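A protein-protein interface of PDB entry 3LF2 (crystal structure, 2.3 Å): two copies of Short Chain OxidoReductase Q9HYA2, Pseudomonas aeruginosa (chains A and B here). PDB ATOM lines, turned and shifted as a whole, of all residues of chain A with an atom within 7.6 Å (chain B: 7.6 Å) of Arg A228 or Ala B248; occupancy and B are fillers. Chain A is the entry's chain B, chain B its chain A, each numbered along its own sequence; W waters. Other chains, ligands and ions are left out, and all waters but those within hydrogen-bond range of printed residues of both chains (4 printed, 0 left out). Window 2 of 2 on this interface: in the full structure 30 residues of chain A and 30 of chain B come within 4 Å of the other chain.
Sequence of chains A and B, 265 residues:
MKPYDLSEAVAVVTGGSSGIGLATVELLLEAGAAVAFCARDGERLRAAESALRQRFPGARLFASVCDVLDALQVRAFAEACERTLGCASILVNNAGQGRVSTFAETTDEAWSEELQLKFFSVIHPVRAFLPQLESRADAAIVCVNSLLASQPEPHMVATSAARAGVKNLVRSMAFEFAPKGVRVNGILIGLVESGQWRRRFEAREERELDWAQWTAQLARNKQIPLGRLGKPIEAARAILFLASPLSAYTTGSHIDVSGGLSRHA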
ATOM      1  N   LEU A 191       5.875  12.506  36.060  1.00  0.00           N
ATOM      2  CA  LEU A 191       7.169  13.026  35.667  1.00  0.00           C
ATOM      3  C   LEU A 191       7.017  13.794  34.345  1.00  0.00           C
ATOM      4  O   LEU A 191       6.691  13.226  33.291  1.00  0.00           O
ATOM      5  CB  LEU A 191       8.193  11.897  35.543  1.00  0.00           C
ATOM      6  CG  LEU A 191       8.847  11.406  36.841  1.00  0.00           C
ATOM      7  CD1 LEU A 191       7.829  11.137  37.935  1.00  0.00           C
ATOM      8  CD2 LEU A 191       9.671  10.171  36.571  1.00  0.00           C
ATOM      9  N   VAL A 192       7.244  15.098  34.428  1.00  0.00           N
ATOM     10  CA  VAL A 192       7.066  16.004  33.311  1.00  0.00           C
ATOM     11  C   VAL A 192       8.352  16.802  33.126  1.00  0.00           C
ATOM     12  O   VAL A 192       8.799  17.459  34.062  1.00  0.00           O
ATOM     13  CB  VAL A 192       5.893  16.966  33.600  1.00  0.00           C
ATOM     14  CG1 VAL A 192       5.795  18.071  32.537  1.00  0.00           C
ATOM     15  CG2 VAL A 192       4.575  16.179  33.731  1.00  0.00           C
ATOM     16  N   GLU A 193       8.963  16.701  31.946  1.00  0.00           N
ATOM     17  CA  GLU A 193      10.119  17.535  31.569  1.00  0.00           C
ATOM     18  C   GLU A 193      10.051  18.930  32.189  1.00  0.00           C
ATOM     19  O   GLU A 193       8.996  19.575  32.207  1.00  0.00           O
ATOM     20  CB  GLU A 193      10.249  17.659  30.041  1.00  0.00           C
ATOM     21  CG  GLU A 193      10.566  16.335  29.341  1.00  0.00           C
ATOM     22  CD  GLU A 193      10.671  16.460  27.829  1.00  0.00           C
ATOM     23  OE1 GLU A 193      10.715  17.596  27.317  1.00  0.00           O
ATOM     24  OE2 GLU A 193      10.713  15.414  27.150  1.00  0.00           O
ATOM     25  N   THR A 215      16.210  10.231  29.197  1.00  0.00           N
ATOM     26  CA  THR A 215      14.817  10.355  29.589  1.00  0.00           C
ATOM     27  C   THR A 215      14.036   9.069  29.344  1.00  0.00           C
ATOM     28  O   THR A 215      13.122   8.748  30.098  1.00  0.00           O
ATOM     29  CB  THR A 215      14.127  11.575  28.939  1.00  0.00           C
ATOM     30  OG1 THR A 215      14.351  11.572  27.518  1.00  0.00           O
ATOM     31  CG2 THR A 215      14.671  12.882  29.562  1.00  0.00           C
ATOM     32  N   ALA A 216      14.404   8.318  28.314  1.00  0.00           N
ATOM     33  CA  ALA A 216      13.740   7.044  28.060  1.00  0.00           C
ATOM     34  C   ALA A 216      14.148   6.029  29.125  1.00  0.00           C
ATOM     35  O   ALA A 216      13.311   5.293  29.647  1.00  0.00           O
ATOM     36  CB  ALA A 216      14.067   6.522  26.673  1.00  0.00           C
ATOM     37  N   LEU A 218      15.061   6.789  32.086  1.00  0.00           N
ATOM     38  CA  LEU A 218      14.391   7.261  33.284  1.00  0.00           C
ATOM     39  C   LEU A 218      12.924   6.836  33.329  1.00  0.00           C
ATOM     40  O   LEU A 218      12.408   6.499  34.386  1.00  0.00           O
ATOM     41  CB  LEU A 218      14.474   8.781  33.347  1.00  0.00           C
ATOM     42  CG  LEU A 218      13.721   9.475  34.480  1.00  0.00           C
ATOM     43  CD1 LEU A 218      14.293   9.030  35.813  1.00  0.00           C
ATOM     44  CD2 LEU A 218      13.810  11.007  34.304  1.00  0.00           C
ATOM     45  N   ALA A 219      12.252   6.886  32.183  1.00  0.00           N
ATOM     46  CA  ALA A 219      10.837   6.549  32.112  1.00  0.00           C
ATOM     47  C   ALA A 219      10.623   5.057  32.321  1.00  0.00           C
ATOM     48  O   ALA A 219       9.674   4.641  32.991  1.00  0.00           O
ATOM     49  CB  ALA A 219      10.252   6.992  30.783  1.00  0.00           C
ATOM     50  N   ARG A 220      11.517   4.259  31.753  1.00  0.00           N
ATOM     51  CA  ARG A 220      11.518   2.830  32.002  1.00  0.00           C
ATOM     52  C   ARG A 220      11.752   2.557  33.486  1.00  0.00           C
ATOM     53  O   ARG A 220      10.975   1.857  34.120  1.00  0.00           O
ATOM     54  CB  ARG A 220      12.580   2.136  31.156  1.00  0.00           C
ATOM     55  CG  ARG A 220      12.305   2.165  29.668  1.00  0.00           C
ATOM     56  CD  ARG A 220      13.211   1.185  28.924  1.00  0.00           C
ATOM     57  NE  ARG A 220      13.062  -0.177  29.441  1.00  0.00           N
ATOM     58  CZ  ARG A 220      12.179  -1.067  28.985  1.00  0.00           C
ATOM     59  NH1 ARG A 220      11.359  -0.750  27.986  1.00  0.00           N
ATOM     60  NH2 ARG A 220      12.116  -2.281  29.529  1.00  0.00           N
ATOM     61  N   GLN A 223       8.865   3.119  35.567  1.00  0.00           N
ATOM     62  CA  GLN A 223       7.724   2.265  35.247  1.00  0.00           C
ATOM     63  C   GLN A 223       6.503   3.079  34.803  1.00  0.00           C
ATOM     64  O   GLN A 223       5.363   2.772  35.162  1.00  0.00           O
ATOM     65  CB  GLN A 223       7.387   1.349  36.435  1.00  0.00           C
ATOM     66  CG  GLN A 223       8.600   0.587  36.956  1.00  0.00           C
ATOM     67  CD  GLN A 223       8.272  -0.286  38.156  1.00  0.00           C
ATOM     68  OE1 GLN A 223       8.062   0.216  39.256  1.00  0.00           O
ATOM     69  NE2 GLN A 223       8.220  -1.598  37.943  1.00  0.00           N
ATOM     70  N   ILE A 224       6.760   4.126  34.023  1.00  0.00           N
ATOM     71  CA  ILE A 224       5.692   4.906  33.431  1.00  0.00           C
ATOM     72  C   ILE A 224       5.095   4.053  32.310  1.00  0.00           C
ATOM     73  O   ILE A 224       5.795   3.686  31.373  1.00  0.00           O
ATOM     74  CB  ILE A 224       6.224   6.248  32.875  1.00  0.00           C
ATOM     75  CG1 ILE A 224       6.941   7.047  33.967  1.00  0.00           C
ATOM     76  CG2 ILE A 224       5.089   7.076  32.281  1.00  0.00           C
ATOM     77  CD1 ILE A 224       7.613   8.315  33.447  1.00  0.00           C
ATOM     78  N   PRO A 225       3.804   3.704  32.417  1.00  0.00           N
ATOM     79  CA  PRO A 225       3.245   2.807  31.390  1.00  0.00           C
ATOM     80  C   PRO A 225       3.366   3.360  29.965  1.00  0.00           C
ATOM     81  O   PRO A 225       3.655   2.588  29.037  1.00  0.00           O
ATOM     82  CB  PRO A 225       1.781   2.653  31.821  1.00  0.00           C
ATOM     83  CG  PRO A 225       1.825   2.822  33.325  1.00  0.00           C
ATOM     84  CD  PRO A 225       2.884   3.890  33.556  1.00  0.00           C
ATOM     85  N   LEU A 226       3.177   4.669  29.796  1.00  0.00           N
ATOM     86  CA  LEU A 226       3.288   5.292  28.473  1.00  0.00           C
ATOM     87  C   LEU A 226       4.740   5.414  28.016  1.00  0.00           C
ATOM     88  O   LEU A 226       5.016   5.829  26.886  1.00  0.00           O
ATOM     89  CB  LEU A 226       2.569   6.652  28.423  1.00  0.00           C
ATOM     90  CG  LEU A 226       1.048   6.577  28.618  1.00  0.00           C
ATOM     91  CD1 LEU A 226       0.389   7.854  28.134  1.00  0.00           C
ATOM     92  CD2 LEU A 226       0.468   5.368  27.890  1.00  0.00           C
ATOM     93  N   GLY A 227       5.662   5.049  28.903  1.00  0.00           N
ATOM     94  CA  GLY A 227       7.041   4.836  28.516  1.00  0.00           C
ATOM     95  C   GLY A 227       7.854   6.072  28.169  1.00  0.00           C
ATOM     96  O   GLY A 227       8.885   5.967  27.514  1.00  0.00           O
ATOM     97  N   ARG A 228       7.403   7.236  28.624  1.00  0.00           N
ATOM     98  CA  ARG A 228       8.143   8.476  28.434  1.00  0.00           C
ATOM     99  C   ARG A 228       7.713   9.482  29.489  1.00  0.00           C
ATOM    100  O   ARG A 228       6.690   9.292  30.158  1.00  0.00           O
ATOM    101  CB  ARG A 228       7.907   9.052  27.031  1.00  0.00           C
ATOM    102  CG  ARG A 228       6.480   9.509  26.807  1.00  0.00           C
ATOM    103  CD  ARG A 228       6.292  10.180  25.450  1.00  0.00           C
ATOM    104  NE  ARG A 228       4.872  10.379  25.182  1.00  0.00           N
ATOM    105  CZ  ARG A 228       4.149  11.376  25.672  1.00  0.00           C
ATOM    106  NH1 ARG A 228       4.728  12.303  26.443  1.00  0.00           N
ATOM    107  NH2 ARG A 228       2.848  11.457  25.380  1.00  0.00           N
ATOM    108  N   LEU A 229       8.515  10.528  29.654  1.00  0.00           N
ATOM    109  CA  LEU A 229       8.173  11.641  30.527  1.00  0.00           C
ATOM    110  C   LEU A 229       7.082  12.487  29.867  1.00  0.00           C
ATOM    111  O   LEU A 229       6.985  12.545  28.638  1.00  0.00           O
ATOM    112  CB  LEU A 229       9.415  12.502  30.799  1.00  0.00           C
ATOM    113  CG  LEU A 229      10.284  12.281  32.051  1.00  0.00           C
ATOM    114  CD1 LEU A 229      10.711  10.825  32.236  1.00  0.00           C
ATOM    115  CD2 LEU A 229      11.509  13.199  32.044  1.00  0.00           C
ATOM    116  N   GLY A 230       6.265  13.147  30.684  1.00  0.00           N
ATOM    117  CA  GLY A 230       5.288  14.097  30.177  1.00  0.00           C
ATOM    118  C   GLY A 230       5.913  15.358  29.587  1.00  0.00           C
ATOM    119  O   GLY A 230       7.077  15.668  29.839  1.00  0.00           O
ATOM    120  N   LYS A 231       5.131  16.074  28.780  1.00  0.00           N
ATOM    121  CA  LYS A 231       5.528  17.368  28.220  1.00  0.00           C
ATOM    122  C   LYS A 231       4.714  18.468  28.882  1.00  0.00           C
ATOM    123  O   LYS A 231       3.528  18.288  29.125  1.00  0.00           O
ATOM    124  CB  LYS A 231       5.266  17.410  26.713  1.00  0.00           C
ATOM    125  CG  LYS A 231       6.039  16.406  25.886  1.00  0.00           C
ATOM    126  CD  LYS A 231       7.451  16.878  25.637  1.00  0.00           C
ATOM    127  CE  LYS A 231       8.142  16.013  24.591  1.00  0.00           C
ATOM    128  NZ  LYS A 231       9.551  16.452  24.338  1.00  0.00           N
ATOM    129  N   GLU A 234       1.391  19.073  27.356  1.00  0.00           N
ATOM    130  CA  GLU A 234       0.368  18.080  27.722  1.00  0.00           C
ATOM    131  C   GLU A 234      -0.322  18.450  29.027  1.00  0.00           C
ATOM    132  O   GLU A 234      -1.547  18.384  29.133  1.00  0.00           O
ATOM    133  CB  GLU A 234       0.960  16.670  27.776  1.00  0.00           C
ATOM    134  CG  GLU A 234       1.445  16.224  26.402  1.00  0.00           C
ATOM    135  CD  GLU A 234       2.270  14.954  26.430  1.00  0.00           C
ATOM    136  OE1 GLU A 234       3.149  14.834  27.306  1.00  0.00           O
ATOM    137  OE2 GLU A 234       2.049  14.087  25.550  1.00  0.00           O
ATOM    138  N   ARG A 237      -2.512  21.460  28.385  1.00  0.00           N
ATOM    139  CA  ARG A 237      -3.752  21.102  27.711  1.00  0.00           C
ATOM    140  C   ARG A 237      -4.847  20.653  28.673  1.00  0.00           C
ATOM    141  O   ARG A 237      -6.007  21.020  28.497  1.00  0.00           O
ATOM    142  CB  ARG A 237      -3.498  20.063  26.613  1.00  0.00           C
ATOM    143  CG  ARG A 237      -2.697  20.639  25.437  1.00  0.00           C
ATOM    144  CD  ARG A 237      -2.561  19.675  24.254  1.00  0.00           C
ATOM    145  NE  ARG A 237      -2.133  20.388  23.051  1.00  0.00           N
ATOM    146  CZ  ARG A 237      -1.113  20.032  22.268  1.00  0.00           C
ATOM    147  NH1 ARG A 237      -0.811  20.768  21.194  1.00  0.00           N
ATOM    148  NH2 ARG A 237      -0.396  18.948  22.554  1.00  0.00           N
ATOM    149  N   VAL A 257      -2.362  13.552  35.033  1.00  0.00           N
ATOM    150  CA  VAL A 257      -1.434  13.736  33.919  1.00  0.00           C
ATOM    151  C   VAL A 257      -0.074  13.102  34.204  1.00  0.00           C
ATOM    152  O   VAL A 257       0.969  13.751  34.106  1.00  0.00           O
ATOM    153  CB  VAL A 257      -1.286  15.212  33.523  1.00  0.00           C
ATOM    154  CG1 VAL A 257      -0.536  15.344  32.189  1.00  0.00           C
ATOM    155  CG2 VAL A 257      -2.648  15.886  33.433  1.00  0.00           C
ATOM    156  N   SER A 258      -0.102  11.813  34.514  1.00  0.00           N
ATOM    157  CA  SER A 258       1.073  11.081  34.978  1.00  0.00           C
ATOM    158  C   SER A 258       1.479   9.929  34.049  1.00  0.00           C
ATOM    159  O   SER A 258       2.391   9.177  34.365  1.00  0.00           O
ATOM    160  CB  SER A 258       0.801  10.512  36.367  1.00  0.00           C
ATOM    161  OG  SER A 258      -0.094   9.407  36.287  1.00  0.00           O
ATOM    162  N   GLY A 259       0.811   9.786  32.910  1.00  0.00           N
ATOM    163  CA  GLY A 259       1.182   8.754  31.954  1.00  0.00           C
ATOM    164  C   GLY A 259       0.937   7.357  32.498  1.00  0.00           C
ATOM    165  O   GLY A 259       1.701   6.439  32.216  1.00  0.00           O
ATOM    166  N   LEU A 261       0.707   6.429  35.952  1.00  0.00           N
ATOM    167  CA  LEU A 261       1.418   6.022  37.178  1.00  0.00           C
ATOM    168  C   LEU A 261       0.512   5.715  38.368  1.00  0.00           C
ATOM    169  O   LEU A 261       0.935   5.068  39.311  1.00  0.00           O
ATOM    170  CB  LEU A 261       2.459   7.055  37.601  1.00  0.00           C
ATOM    171  CG  LEU A 261       3.814   7.048  36.899  1.00  0.00           C
ATOM    172  CD1 LEU A 261       4.592   8.289  37.325  1.00  0.00           C
ATOM    173  CD2 LEU A 261       4.612   5.780  37.184  1.00  0.00           C
ATOM    174  N   ASP B 138      -2.286   7.265  18.210  1.00  0.00           N
ATOM    175  CA  ASP B 138      -3.270   8.098  18.898  1.00  0.00           C
ATOM    176  C   ASP B 138      -4.507   7.267  19.245  1.00  0.00           C
ATOM    177  O   ASP B 138      -5.626   7.783  19.222  1.00  0.00           O
ATOM    178  CB  ASP B 138      -3.677   9.303  18.025  1.00  0.00           C
ATOM    179  CG  ASP B 138      -2.474  10.112  17.509  1.00  0.00           C
ATOM    180  OD1 ASP B 138      -1.382  10.076  18.120  1.00  0.00           O
ATOM    181  OD2 ASP B 138      -2.629  10.806  16.484  1.00  0.00           O
ATOM    182  N   ARG B 183      -4.435   4.186  24.981  1.00  0.00           N
ATOM    183  CA  ARG B 183      -4.806   4.768  26.262  1.00  0.00           C
ATOM    184  C   ARG B 183      -6.233   4.365  26.628  1.00  0.00           C
ATOM    185  O   ARG B 183      -7.068   4.130  25.746  1.00  0.00           O
ATOM    186  CB  ARG B 183      -4.687   6.288  26.221  1.00  0.00           C
ATOM    187  CG  ARG B 183      -3.294   6.805  25.899  1.00  0.00           C
ATOM    188  CD  ARG B 183      -3.239   8.344  25.928  1.00  0.00           C
ATOM    189  NE  ARG B 183      -4.101   8.948  24.917  1.00  0.00           N
ATOM    190  CZ  ARG B 183      -5.256   9.561  25.171  1.00  0.00           C
ATOM    191  NH1 ARG B 183      -5.711   9.680  26.417  1.00  0.00           N
ATOM    192  NH2 ARG B 183      -5.959  10.073  24.160  1.00  0.00           N
ATOM    193  N   PHE B 241     -12.165  15.171  24.969  1.00  0.00           N
ATOM    194  CA  PHE B 241     -10.828  15.459  25.456  1.00  0.00           C
ATOM    195  C   PHE B 241     -10.054  14.138  25.687  1.00  0.00           C
ATOM    196  O   PHE B 241      -8.925  13.982  25.211  1.00  0.00           O
ATOM    197  CB  PHE B 241     -10.907  16.321  26.717  1.00  0.00           C
ATOM    198  CG  PHE B 241      -9.585  16.519  27.391  1.00  0.00           C
ATOM    199  CD1 PHE B 241      -8.645  17.378  26.858  1.00  0.00           C
ATOM    200  CD2 PHE B 241      -9.283  15.835  28.562  1.00  0.00           C
ATOM    201  CE1 PHE B 241      -7.431  17.547  27.481  1.00  0.00           C
ATOM    202  CE2 PHE B 241      -8.081  15.989  29.184  1.00  0.00           C
ATOM    203  CZ  PHE B 241      -7.142  16.846  28.650  1.00  0.00           C
ATOM    204  N   LEU B 242     -10.685  13.177  26.368  1.00  0.00           N
ATOM    205  CA  LEU B 242     -10.049  11.886  26.665  1.00  0.00           C
ATOM    206  C   LEU B 242      -9.780  11.031  25.430  1.00  0.00           C
ATOM    207  O   LEU B 242      -8.809  10.278  25.395  1.00  0.00           O
ATOM    208  CB  LEU B 242     -10.910  11.089  27.620  1.00  0.00           C
ATOM    209  CG  LEU B 242     -10.871  11.558  29.073  1.00  0.00           C
ATOM    210  CD1 LEU B 242     -11.841  10.758  29.924  1.00  0.00           C
ATOM    211  CD2 LEU B 242      -9.449  11.459  29.632  1.00  0.00           C
ATOM    212  N   SER B 244      -9.178  12.224  22.414  1.00  0.00           N
ATOM    213  CA  SER B 244      -8.288  12.967  21.524  1.00  0.00           C
ATOM    214  C   SER B 244      -6.831  13.032  22.013  1.00  0.00           C
ATOM    215  O   SER B 244      -6.552  12.793  23.181  1.00  0.00           O
ATOM    216  CB  SER B 244      -8.812  14.394  21.367  1.00  0.00           C
ATOM    217  OG  SER B 244      -8.378  15.223  22.439  1.00  0.00           O
ATOM    218  N   PRO B 245      -5.900  13.367  21.109  1.00  0.00           N
ATOM    219  CA  PRO B 245      -4.486  13.576  21.438  1.00  0.00           C
ATOM    220  C   PRO B 245      -4.239  14.727  22.412  1.00  0.00           C
ATOM    221  O   PRO B 245      -3.082  14.913  22.811  1.00  0.00           O
ATOM    222  CB  PRO B 245      -3.850  13.905  20.075  1.00  0.00           C
ATOM    223  CG  PRO B 245      -4.760  13.276  19.076  1.00  0.00           C
ATOM    224  CD  PRO B 245      -6.139  13.435  19.653  1.00  0.00           C
ATOM    225  N   LEU B 246      -5.277  15.482  22.776  1.00  0.00           N
ATOM    226  CA  LEU B 246      -5.119  16.548  23.772  1.00  0.00           C
ATOM    227  C   LEU B 246      -4.768  15.998  25.181  1.00  0.00           C
ATOM    228  O   LEU B 246      -4.203  16.717  26.013  1.00  0.00           O
ATOM    229  CB  LEU B 246      -6.366  17.443  23.825  1.00  0.00           C
ATOM    230  CG  LEU B 246      -6.634  18.307  22.583  1.00  0.00           C
ATOM    231  CD1 LEU B 246      -7.869  19.201  22.747  1.00  0.00           C
ATOM    232  CD2 LEU B 246      -5.406  19.154  22.230  1.00  0.00           C
ATOM    233  N   SER B 247      -5.091  14.724  25.422  1.00  0.00           N
ATOM    234  CA  SER B 247      -4.840  14.058  26.701  1.00  0.00           C
ATOM    235  C   SER B 247      -3.850  12.897  26.554  1.00  0.00           C
ATOM    236  O   SER B 247      -3.975  11.872  27.226  1.00  0.00           O
ATOM    237  CB  SER B 247      -6.160  13.530  27.255  1.00  0.00           C
ATOM    238  OG  SER B 247      -6.779  12.664  26.315  1.00  0.00           O
ATOM    239  N   ALA B 248      -2.864  13.074  25.677  1.00  0.00           N
ATOM    240  CA  ALA B 248      -1.932  12.013  25.273  1.00  0.00           C
ATOM    241  C   ALA B 248      -1.084  11.431  26.407  1.00  0.00           C
ATOM    242  O   ALA B 248      -0.382  10.430  26.214  1.00  0.00           O
ATOM    243  CB  ALA B 248      -1.007  12.535  24.180  1.00  0.00           C
ATOM    244  N   TYR B 249      -1.094  12.083  27.561  1.00  0.00           N
ATOM    245  CA  TYR B 249      -0.321  11.592  28.703  1.00  0.00           C
ATOM    246  C   TYR B 249      -1.235  11.183  29.853  1.00  0.00           C
ATOM    247  O   TYR B 249      -0.810  11.076  31.004  1.00  0.00           O
ATOM    248  CB  TYR B 249       0.665  12.651  29.171  1.00  0.00           C
ATOM    249  CG  TYR B 249       1.852  12.095  29.903  1.00  0.00           C
ATOM    250  CD1 TYR B 249       2.715  11.201  29.276  1.00  0.00           C
ATOM    251  CD2 TYR B 249       2.128  12.482  31.213  1.00  0.00           C
ATOM    252  CE1 TYR B 249       3.824  10.711  29.937  1.00  0.00           C
ATOM    253  CE2 TYR B 249       3.230  11.984  31.886  1.00  0.00           C
ATOM    254  CZ  TYR B 249       4.072  11.103  31.243  1.00  0.00           C
ATOM    255  OH  TYR B 249       5.166  10.602  31.899  1.00  0.00           O
ATOM    256  N   THR B 250      -2.496  10.936  29.522  1.00  0.00           N
ATOM    257  CA  THR B 250      -3.485  10.568  30.504  1.00  0.00           C
ATOM    258  C   THR B 250      -3.989   9.171  30.199  1.00  0.00           C
ATOM    259  O   THR B 250      -4.552   8.922  29.126  1.00  0.00           O
ATOM    260  CB  THR B 250      -4.690  11.507  30.444  1.00  0.00           C
ATOM    261  OG1 THR B 250      -4.307  12.804  30.894  1.00  0.00           O
ATOM    262  CG2 THR B 250      -5.850  10.969  31.308  1.00  0.00           C
ATOM    263  N   THR B 251      -3.814   8.259  31.143  1.00  0.00           N
ATOM    264  CA  THR B 251      -4.339   6.919  30.942  1.00  0.00           C
ATOM    265  C   THR B 251      -4.617   6.247  32.292  1.00  0.00           C
ATOM    266  O   THR B 251      -3.985   6.572  33.306  1.00  0.00           O
ATOM    267  CB  THR B 251      -3.384   6.080  30.074  1.00  0.00           C
ATOM    268  OG1 THR B 251      -4.084   4.958  29.529  1.00  0.00           O
ATOM    269  CG2 THR B 251      -2.207   5.597  30.902  1.00  0.00           C
HETATM  270  O   HOH W   1      -2.432   7.086  36.198  1.00  0.00           O
HETATM  271  O   HOH W   2      -2.376   8.896  33.557  1.00  0.00           O
HETATM  272  O   HOH W   3      -3.549  16.867  28.526  1.00  0.00           O
HETATM  273  O   HOH W   4       4.818  10.466  34.698  1.00  0.00           O
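The backbone NH (N) of Gly A230 lies within hydrogen-bond range of the side-chain hydroxyl (OH) of Tyr B249 (3.0 Å). The side-chain hydroxyl (OH) of Tyr B249 is in hydrogen-bond range of the backbone carbonyl oxygen (O) of Arg A228 (2.7 Å). The backbone NH (N) of Gly A259 sits at hydrogen-bond distance from the backbone carbonyl oxygen (O) of Tyr B249, at 2.8 Å. OH of Tyr B249 is in hydrogen-bond range of O of Leu A191 (3.3 Å). The guanidinium group (NH2) of Arg A228 sits at hydrogen-bond distance from the backbone carbonyl oxygen (O) of Ala B248 (3.5 Å).
The side-chain hydroxyl (OG) of Ser A258 is in hydrogen-bond range of the backbone NH (N) of Leu A261 (3.1 Å). The backbone carbonyl oxygen (O) of Ala A219 sits at hydrogen-bond distance from the backbone NH (N) of Ile A224. The backbone NH (N) of Leu A226 lies within hydrogen-bond range of the backbone carbonyl oxygen (O) of Gly A259, 3.3 Å away. N of Gly A230 lies within hydrogen-bond range of O of Leu A191 (2.6 Å). The backbone NH (N) of Glu A193 is in hydrogen-bond range of the backbone carbonyl oxygen (O) of Gly A230 (3.0 Å). The side-chain carboxylate (OE1) of Glu A234 lies within hydrogen-bond range of the backbone NH (N) of Lys A231, at 2.8 Å.
Ile A224 touches Tyr B249. O of Ala B248 touches CD1 of Leu A226 (3.3 Å). Tyr B249 touches Leu A226. C of Leu A229 touches OH of Tyr B249, 3.4 Å away. CB of Ala B248 touches OE2 of Glu A234 (3.7 Å). Glu A234 touches Tyr B249. Phe B241 touches Arg A237 (CE1 to O, 3.9 Å). CB of Arg A237 touches O of Leu B246, at 3.5 Å. Tyr B249 touches Ser A258 (CE2 to C, 3.5 Å). Gly A259 touches Thr B251 (C to CG2, 3.9 Å).
Of chain B, only Ala B248 and Tyr B249 come within 4 Å of Arg A228. Ala B248 touches just these residues of chain A: Leu A226, Arg A228 and Glu A234. No residue of chain B comes within 4 Å of Gly A227. Of the printed residues of chain B, Gly A230 touches Tyr B249 (3.0 Å). Of the printed residues of chain A, Tyr B249 touches Leu A191, Ile A224, Leu A226, Arg A228, Leu A229, Gly A230, Glu A234, Val A257, Ser A258 and Gly A259. The nearest residue of chain B that does not touch Arg A228 is Thr B250 (6.8 Å). The nearest residue of chain A that does not touch Ala B248 is Gly A259 (6.2 Å).
Of the 12 printed residues of chain B, 5 touch a printed residue of chain A. Printed residues of chain B that touch a printed residue of chain A: Phe B241, Leu B246, Ala B248, Tyr B249 and Thr B251. Hydrophobic or aromatic side chains of chain B within 4 Å of the printed part of chain A: Phe B241, Leu B246, Ala B248 and Tyr B249. Along chain B the printed residues that touch a printed residue of chain A span positions 241 to 251. Of the 23 printed residues of chain A, 11 touch a printed residue of chain B. Hydrophobic or aromatic side chains of chain A that line the printed part of chain B: Ile A224 and Leu A226. Among the printed residues, no Asp or Glu carboxylate lies within 4 Å of a Lys or Arg side-chain nitrogen of the other chain.
No position is printed for both chains.
Water W3 bridges O of Glu A234 (2.6 Å) and O of Leu B246 (2.6 Å). Water W4 lies within hydrogen-bond range of the backbone NH of Leu A191 (2.7 Å), the backbone carbonyl oxygen of Ser A258 (2.8 Å) and the side-chain hydroxyl of Tyr B249 (2.8 Å). Water W2 lies within hydrogen-bond range of the backbone carbonyl oxygen of Thr B251 (2.8 Å) and the backbone NH of Gly A259 (3.4 Å). Water W1 lies within hydrogen-bond range of the backbone NH of Leu A261 (3.2 Å), the side-chain hydroxyl of Ser A258 (3.3 Å) and the backbone carbonyl oxygen of Thr B251 (3.3 Å).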
